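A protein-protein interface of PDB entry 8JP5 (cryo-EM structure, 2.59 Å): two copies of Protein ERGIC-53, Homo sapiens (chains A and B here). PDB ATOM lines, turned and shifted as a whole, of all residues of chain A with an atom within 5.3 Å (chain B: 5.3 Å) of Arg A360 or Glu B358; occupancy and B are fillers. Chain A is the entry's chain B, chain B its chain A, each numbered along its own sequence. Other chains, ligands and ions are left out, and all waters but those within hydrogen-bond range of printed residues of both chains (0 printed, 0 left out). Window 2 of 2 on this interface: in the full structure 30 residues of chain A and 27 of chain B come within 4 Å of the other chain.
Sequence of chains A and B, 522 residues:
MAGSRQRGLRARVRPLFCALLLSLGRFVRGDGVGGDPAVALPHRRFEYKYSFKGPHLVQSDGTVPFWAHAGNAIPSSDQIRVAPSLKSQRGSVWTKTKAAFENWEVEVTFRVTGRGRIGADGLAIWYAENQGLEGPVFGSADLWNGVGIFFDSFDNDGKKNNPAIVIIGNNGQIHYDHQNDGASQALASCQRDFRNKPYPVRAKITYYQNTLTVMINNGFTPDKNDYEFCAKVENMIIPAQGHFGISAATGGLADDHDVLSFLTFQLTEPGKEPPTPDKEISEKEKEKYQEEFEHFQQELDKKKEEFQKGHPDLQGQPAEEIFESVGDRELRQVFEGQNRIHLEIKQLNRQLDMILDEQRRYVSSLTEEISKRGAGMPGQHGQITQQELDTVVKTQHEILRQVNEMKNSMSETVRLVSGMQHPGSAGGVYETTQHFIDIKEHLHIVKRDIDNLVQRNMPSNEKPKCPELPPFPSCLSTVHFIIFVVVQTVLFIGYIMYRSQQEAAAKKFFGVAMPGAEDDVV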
ATOM      1  N   ILE A 355      14.108 -14.455  -4.451  1.00  0.00           N
ATOM      2  CA  ILE A 355      14.587 -13.461  -3.492  1.00  0.00           C
ATOM      3  C   ILE A 355      13.475 -12.477  -3.143  1.00  0.00           C
ATOM      4  O   ILE A 355      13.222 -12.200  -1.965  1.00  0.00           O
ATOM      5  CB  ILE A 355      15.828 -12.742  -4.059  1.00  0.00           C
ATOM      6  CG1 ILE A 355      17.105 -13.496  -3.693  1.00  0.00           C
ATOM      7  CG2 ILE A 355      15.942 -11.323  -3.533  1.00  0.00           C
ATOM      8  CD1 ILE A 355      17.389 -13.492  -2.204  1.00  0.00           C
ATOM      9  N   LEU A 356      12.804 -11.935  -4.169  1.00  0.00           N
ATOM     10  CA  LEU A 356      11.623 -11.089  -4.021  1.00  0.00           C
ATOM     11  C   LEU A 356      10.598 -11.684  -3.066  1.00  0.00           C
ATOM     12  O   LEU A 356      10.207 -11.055  -2.070  1.00  0.00           O
ATOM     13  CB  LEU A 356      10.974 -10.874  -5.394  1.00  0.00           C
ATOM     14  CG  LEU A 356       9.862  -9.829  -5.601  1.00  0.00           C
ATOM     15  CD1 LEU A 356       9.998  -8.611  -4.685  1.00  0.00           C
ATOM     16  CD2 LEU A 356       9.667  -9.426  -7.072  1.00  0.00           C
ATOM     17  N   ASP A 357      10.141 -12.896  -3.387  1.00  0.00           N
ATOM     18  CA  ASP A 357       9.090 -13.530  -2.598  1.00  0.00           C
ATOM     19  C   ASP A 357       9.529 -13.710  -1.150  1.00  0.00           C
ATOM     20  O   ASP A 357       8.760 -13.435  -0.220  1.00  0.00           O
ATOM     21  CB  ASP A 357       8.695 -14.872  -3.219  1.00  0.00           C
ATOM     22  CG  ASP A 357       8.019 -15.800  -2.222  1.00  0.00           C
ATOM     23  OD1 ASP A 357       6.919 -15.456  -1.738  1.00  0.00           O
ATOM     24  OD2 ASP A 357       8.578 -16.878  -1.932  1.00  0.00           O
ATOM     25  N   GLU A 358      10.771 -14.159  -0.941  1.00  0.00           N
ATOM     26  CA  GLU A 358      11.261 -14.394   0.414  1.00  0.00           C
ATOM     27  C   GLU A 358      11.363 -13.094   1.213  1.00  0.00           C
ATOM     28  O   GLU A 358      10.995 -13.054   2.398  1.00  0.00           O
ATOM     29  CB  GLU A 358      12.603 -15.122   0.360  1.00  0.00           C
ATOM     30  CG  GLU A 358      13.338 -15.185   1.679  1.00  0.00           C
ATOM     31  CD  GLU A 358      14.552 -16.083   1.610  1.00  0.00           C
ATOM     32  OE1 GLU A 358      14.794 -16.675   0.537  1.00  0.00           O
ATOM     33  OE2 GLU A 358      15.254 -16.204   2.633  1.00  0.00           O
ATOM     34  N   GLN A 359      11.867 -12.018   0.590  1.00  0.00           N
ATOM     35  CA  GLN A 359      11.894 -10.730   1.284  1.00  0.00           C
ATOM     36  C   GLN A 359      10.491 -10.275   1.655  1.00  0.00           C
ATOM     37  O   GLN A 359      10.286  -9.712   2.732  1.00  0.00           O
ATOM     38  CB  GLN A 359      12.584  -9.630   0.466  1.00  0.00           C
ATOM     39  CG  GLN A 359      13.963  -9.914  -0.099  1.00  0.00           C
ATOM     40  CD  GLN A 359      14.941 -10.438   0.929  1.00  0.00           C
ATOM     41  OE1 GLN A 359      15.266  -9.756   1.903  1.00  0.00           O
ATOM     42  NE2 GLN A 359      15.447 -11.641   0.696  1.00  0.00           N
ATOM     43  N   ARG A 360       9.512 -10.489   0.771  1.00  0.00           N
ATOM     44  CA  ARG A 360       8.142 -10.092   1.104  1.00  0.00           C
ATOM     45  C   ARG A 360       7.558 -10.928   2.243  1.00  0.00           C
ATOM     46  O   ARG A 360       6.831 -10.397   3.096  1.00  0.00           O
ATOM     47  CB  ARG A 360       7.254 -10.146  -0.138  1.00  0.00           C
ATOM     48  CG  ARG A 360       7.709  -9.256  -1.303  1.00  0.00           C
ATOM     49  CD  ARG A 360       7.589  -7.748  -0.981  1.00  0.00           C
ATOM     50  NE  ARG A 360       8.631  -7.185  -0.124  1.00  0.00           N
ATOM     51  CZ  ARG A 360       9.916  -7.091  -0.442  1.00  0.00           C
ATOM     52  NH1 ARG A 360      10.360  -7.427  -1.641  1.00  0.00           N
ATOM     53  NH2 ARG A 360      10.774  -6.619   0.458  1.00  0.00           N
ATOM     54  N   ARG A 361       7.853 -12.234   2.276  1.00  0.00           N
ATOM     55  CA  ARG A 361       7.427 -13.059   3.409  1.00  0.00           C
ATOM     56  C   ARG A 361       8.032 -12.560   4.714  1.00  0.00           C
ATOM     57  O   ARG A 361       7.361 -12.539   5.754  1.00  0.00           O
ATOM     58  CB  ARG A 361       7.789 -14.535   3.195  1.00  0.00           C
ATOM     59  CG  ARG A 361       7.341 -15.205   1.896  1.00  0.00           C
ATOM     60  CD  ARG A 361       5.831 -15.508   1.822  1.00  0.00           C
ATOM     61  NE  ARG A 361       4.943 -14.350   1.847  1.00  0.00           N
ATOM     62  CZ  ARG A 361       4.922 -13.379   0.942  1.00  0.00           C
ATOM     63  NH1 ARG A 361       5.687 -13.414  -0.137  1.00  0.00           N
ATOM     64  NH2 ARG A 361       4.099 -12.349   1.119  1.00  0.00           N
ATOM     65  N   TYR A 362       9.313 -12.181   4.686  1.00  0.00           N
ATOM     66  CA  TYR A 362       9.919 -11.590   5.878  1.00  0.00           C
ATOM     67  C   TYR A 362       9.283 -10.245   6.213  1.00  0.00           C
ATOM     68  O   TYR A 362       9.151  -9.886   7.390  1.00  0.00           O
ATOM     69  CB  TYR A 362      11.427 -11.428   5.696  1.00  0.00           C
ATOM     70  CG  TYR A 362      12.104 -10.884   6.933  1.00  0.00           C
ATOM     71  CD1 TYR A 362      12.062 -11.590   8.130  1.00  0.00           C
ATOM     72  CD2 TYR A 362      12.764  -9.662   6.917  1.00  0.00           C
ATOM     73  CE1 TYR A 362      12.669 -11.101   9.271  1.00  0.00           C
ATOM     74  CE2 TYR A 362      13.377  -9.163   8.057  1.00  0.00           C
ATOM     75  CZ  TYR A 362      13.323  -9.890   9.231  1.00  0.00           C
ATOM     76  OH  TYR A 362      13.926  -9.408  10.371  1.00  0.00           O
ATOM     77  N   VAL A 363       8.913  -9.481   5.183  1.00  0.00           N
ATOM     78  CA  VAL A 363       8.280  -8.179   5.372  1.00  0.00           C
ATOM     79  C   VAL A 363       6.953  -8.332   6.105  1.00  0.00           C
ATOM     80  O   VAL A 363       6.604  -7.514   6.968  1.00  0.00           O
ATOM     81  CB  VAL A 363       8.111  -7.481   4.005  1.00  0.00           C
ATOM     82  CG1 VAL A 363       6.760  -6.770   3.887  1.00  0.00           C
ATOM     83  CG2 VAL A 363       9.258  -6.517   3.752  1.00  0.00           C
ATOM     84  N   SER A 364       6.201  -9.389   5.779  1.00  0.00           N
ATOM     85  CA  SER A 364       4.888  -9.598   6.383  1.00  0.00           C
ATOM     86  C   SER A 364       4.985  -9.759   7.897  1.00  0.00           C
ATOM     87  O   SER A 364       4.078  -9.346   8.632  1.00  0.00           O
ATOM     88  CB  SER A 364       4.215 -10.818   5.753  1.00  0.00           C
ATOM     89  OG  SER A 364       2.973 -11.094   6.375  1.00  0.00           O
ATOM     90  N   MET B 354      13.975  -2.317  -8.412  1.00  0.00           N
ATOM     91  CA  MET B 354      12.871  -2.215  -7.466  1.00  0.00           C
ATOM     92  C   MET B 354      13.271  -2.803  -6.120  1.00  0.00           C
ATOM     93  O   MET B 354      12.864  -2.286  -5.072  1.00  0.00           O
ATOM     94  CB  MET B 354      11.590  -2.855  -8.021  1.00  0.00           C
ATOM     95  CG  MET B 354      11.588  -4.355  -8.233  1.00  0.00           C
ATOM     96  SD  MET B 354      11.198  -5.290  -6.738  1.00  0.00           S
ATOM     97  CE  MET B 354      12.145  -6.782  -7.009  1.00  0.00           C
ATOM     98  N   ILE B 355      14.115  -3.846  -6.117  1.00  0.00           N
ATOM     99  CA  ILE B 355      14.556  -4.383  -4.830  1.00  0.00           C
ATOM    100  C   ILE B 355      15.515  -3.406  -4.174  1.00  0.00           C
ATOM    101  O   ILE B 355      15.871  -3.550  -2.997  1.00  0.00           O
ATOM    102  CB  ILE B 355      15.149  -5.802  -4.958  1.00  0.00           C
ATOM    103  CG1 ILE B 355      14.981  -6.534  -3.625  1.00  0.00           C
ATOM    104  CG2 ILE B 355      16.624  -5.770  -5.301  1.00  0.00           C
ATOM    105  CD1 ILE B 355      14.626  -7.977  -3.767  1.00  0.00           C
ATOM    106  N   LEU B 356      15.954  -2.401  -4.923  1.00  0.00           N
ATOM    107  CA  LEU B 356      16.478  -1.200  -4.299  1.00  0.00           C
ATOM    108  C   LEU B 356      15.340  -0.415  -3.652  1.00  0.00           C
ATOM    109  O   LEU B 356      15.191  -0.413  -2.419  1.00  0.00           O
ATOM    110  CB  LEU B 356      17.198  -0.363  -5.366  1.00  0.00           C
ATOM    111  CG  LEU B 356      18.274   0.689  -5.118  1.00  0.00           C
ATOM    112  CD1 LEU B 356      17.669   1.984  -4.609  1.00  0.00           C
ATOM    113  CD2 LEU B 356      19.375   0.198  -4.189  1.00  0.00           C
ATOM    114  N   ASP B 357      14.445   0.119  -4.492  1.00  0.00           N
ATOM    115  CA  ASP B 357      13.591   1.245  -4.120  1.00  0.00           C
ATOM    116  C   ASP B 357      12.729   0.930  -2.904  1.00  0.00           C
ATOM    117  O   ASP B 357      12.870   1.563  -1.849  1.00  0.00           O
ATOM    118  CB  ASP B 357      12.711   1.643  -5.310  1.00  0.00           C
ATOM    119  CG  ASP B 357      13.518   2.024  -6.536  1.00  0.00           C
ATOM    120  OD1 ASP B 357      14.763   2.002  -6.464  1.00  0.00           O
ATOM    121  OD2 ASP B 357      12.909   2.360  -7.573  1.00  0.00           O
ATOM    122  N   GLU B 358      11.863  -0.085  -3.025  1.00  0.00           N
ATOM    123  CA  GLU B 358      10.920  -0.388  -1.951  1.00  0.00           C
ATOM    124  C   GLU B 358      11.654  -0.721  -0.662  1.00  0.00           C
ATOM    125  O   GLU B 358      11.208  -0.335   0.426  1.00  0.00           O
ATOM    126  CB  GLU B 358       9.975  -1.523  -2.374  1.00  0.00           C
ATOM    127  CG  GLU B 358      10.586  -2.912  -2.673  1.00  0.00           C
ATOM    128  CD  GLU B 358      10.982  -3.707  -1.432  1.00  0.00           C
ATOM    129  OE1 GLU B 358      10.134  -3.861  -0.526  1.00  0.00           O
ATOM    130  OE2 GLU B 358      12.138  -4.178  -1.366  1.00  0.00           O
ATOM    131  N   GLN B 359      12.819  -1.373  -0.775  1.00  0.00           N
ATOM    132  CA  GLN B 359      13.572  -1.734   0.418  1.00  0.00           C
ATOM    133  C   GLN B 359      13.960  -0.488   1.194  1.00  0.00           C
ATOM    134  O   GLN B 359      13.788  -0.424   2.419  1.00  0.00           O
ATOM    135  CB  GLN B 359      14.809  -2.543   0.035  1.00  0.00           C
ATOM    136  CG  GLN B 359      15.796  -2.685   1.169  1.00  0.00           C
ATOM    137  CD  GLN B 359      16.966  -1.741   1.013  1.00  0.00           C
ATOM    138  OE1 GLN B 359      16.998  -0.927   0.089  1.00  0.00           O
ATOM    139  NE2 GLN B 359      17.913  -1.809   1.938  1.00  0.00           N
ATOM    140  N   ARG B 360      14.430   0.537   0.473  1.00  0.00           N
ATOM    141  CA  ARG B 360      14.754   1.816   1.090  1.00  0.00           C
ATOM    142  C   ARG B 360      13.581   2.349   1.897  1.00  0.00           C
ATOM    143  O   ARG B 360      13.751   2.773   3.047  1.00  0.00           O
ATOM    144  CB  ARG B 360      15.181   2.822   0.020  1.00  0.00           C
ATOM    145  CG  ARG B 360      16.612   2.655  -0.457  1.00  0.00           C
ATOM    146  CD  ARG B 360      17.031   3.837  -1.332  1.00  0.00           C
ATOM    147  NE  ARG B 360      18.434   3.829  -1.741  1.00  0.00           N
ATOM    148  CZ  ARG B 360      19.476   3.888  -0.918  1.00  0.00           C
ATOM    149  NH1 ARG B 360      19.323   4.018   0.391  1.00  0.00           N
ATOM    150  NH2 ARG B 360      20.704   3.856  -1.424  1.00  0.00           N
ATOM    151  N   ARG B 361      12.370   2.272   1.329  1.00  0.00           N
ATOM    152  CA  ARG B 361      11.185   2.719   2.051  1.00  0.00           C
ATOM    153  C   ARG B 361      11.050   1.971   3.369  1.00  0.00           C
ATOM    154  O   ARG B 361      10.923   2.585   4.437  1.00  0.00           O
ATOM    155  CB  ARG B 361       9.935   2.520   1.191  1.00  0.00           C
ATOM    156  CG  ARG B 361       9.433   3.769   0.473  1.00  0.00           C
ATOM    157  CD  ARG B 361      10.423   4.264  -0.582  1.00  0.00           C
ATOM    158  NE  ARG B 361      10.490   3.419  -1.773  1.00  0.00           N
ATOM    159  CZ  ARG B 361       9.499   3.207  -2.630  1.00  0.00           C
ATOM    160  NH1 ARG B 361       8.324   3.803  -2.502  1.00  0.00           N
ATOM    161  NH2 ARG B 361       9.699   2.387  -3.658  1.00  0.00           N
ATOM    162  N   TYR B 362      11.151   0.642   3.317  1.00  0.00           N
ATOM    163  CA  TYR B 362      11.082  -0.152   4.537  1.00  0.00           C
ATOM    164  C   TYR B 362      12.275   0.141   5.436  1.00  0.00           C
ATOM    165  O   TYR B 362      12.155   0.117   6.667  1.00  0.00           O
ATOM    166  CB  TYR B 362      10.986  -1.640   4.196  1.00  0.00           C
ATOM    167  CG  TYR B 362       9.632  -2.053   3.646  1.00  0.00           C
ATOM    168  CD1 TYR B 362       9.151  -1.529   2.450  1.00  0.00           C
ATOM    169  CD2 TYR B 362       8.831  -2.964   4.323  1.00  0.00           C
ATOM    170  CE1 TYR B 362       7.922  -1.894   1.946  1.00  0.00           C
ATOM    171  CE2 TYR B 362       7.594  -3.336   3.824  1.00  0.00           C
ATOM    172  CZ  TYR B 362       7.148  -2.799   2.634  1.00  0.00           C
ATOM    173  OH  TYR B 362       5.923  -3.164   2.128  1.00  0.00           O
ATOM    174  N   VAL B 363      13.436   0.420   4.840  1.00  0.00           N
ATOM    175  CA  VAL B 363      14.565   0.909   5.626  1.00  0.00           C
ATOM    176  C   VAL B 363      14.222   2.259   6.244  1.00  0.00           C
ATOM    177  O   VAL B 363      14.469   2.499   7.432  1.00  0.00           O
ATOM    178  CB  VAL B 363      15.836   0.979   4.760  1.00  0.00           C
ATOM    179  CG1 VAL B 363      16.847   1.954   5.356  1.00  0.00           C
ATOM    180  CG2 VAL B 363      16.444  -0.405   4.619  1.00  0.00           C
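Arg A360 touches just one residue of chain B: Glu B358 (3.0 Å).
Glu B358 touches just one residue of chain A: Arg A360.
Of the printed residues of chain A, Ile B355 touches Ile A355.
Of the printed residues of chain A, Met B354 touches Leu A356 (3.6 Å).
Of the printed residues of chain B, Ile A355 touches Ile B355 (3.6 Å).
Of the printed residues of chain A, Tyr B362 touches Val A363 (3.5 Å).
Arg A361 touches none of the printed residues of chain B.
The nearest residue of chain B that does not touch Arg A360 is Ile B355 (4.8 Å).
The guanidinium group (NH2) of Arg A360 lies within salt-bridge range of the side-chain carboxylate (OE1) of Glu B358 (3.0 Å).
Among the printed residues, pairs that only touch across the chains: Ile A355 with Ile B355 (3.6 Å), Leu A356 with Met B354 (3.6 Å) and Val A363 with Tyr B362 (3.5 Å).
Of the 10 printed residues of chain A, 4 touch a printed residue of chain B.
Printed residues of chain A that touch a printed residue of chain B: Ile A355, Leu A356, Arg A360 and Val A363.
Of the 10 printed residues of chain B, 4 touch a printed residue of chain A.
Hydrophobic or aromatic side chains of chain B that line the printed part of chain A: Met B354, Ile B355 and Tyr B362.
Along chain B the printed residues that touch a printed residue of chain A span positions 354 to 362.
Among the printed residues, Asp or Glu carboxylates within 4 Å of a Lys or Arg side-chain nitrogen of the other chain: Arg A360 with Glu B358 (3.0 Å).
Ile B355 touches its own counterpart, Ile A355.
Arg A360 touches Glu B358, but with the chains exchanged Glu A358 does not touch Arg B360 (14.0 Å).
Val A363 touches Tyr B362, but with the chains exchanged Tyr A362 does not touch Val B363 (9.9 Å).
9 positions are printed for both chains.
Of the 4 pairs that touch across the chains among the printed residues, 1 has its exchanged pair printed and touching as well.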
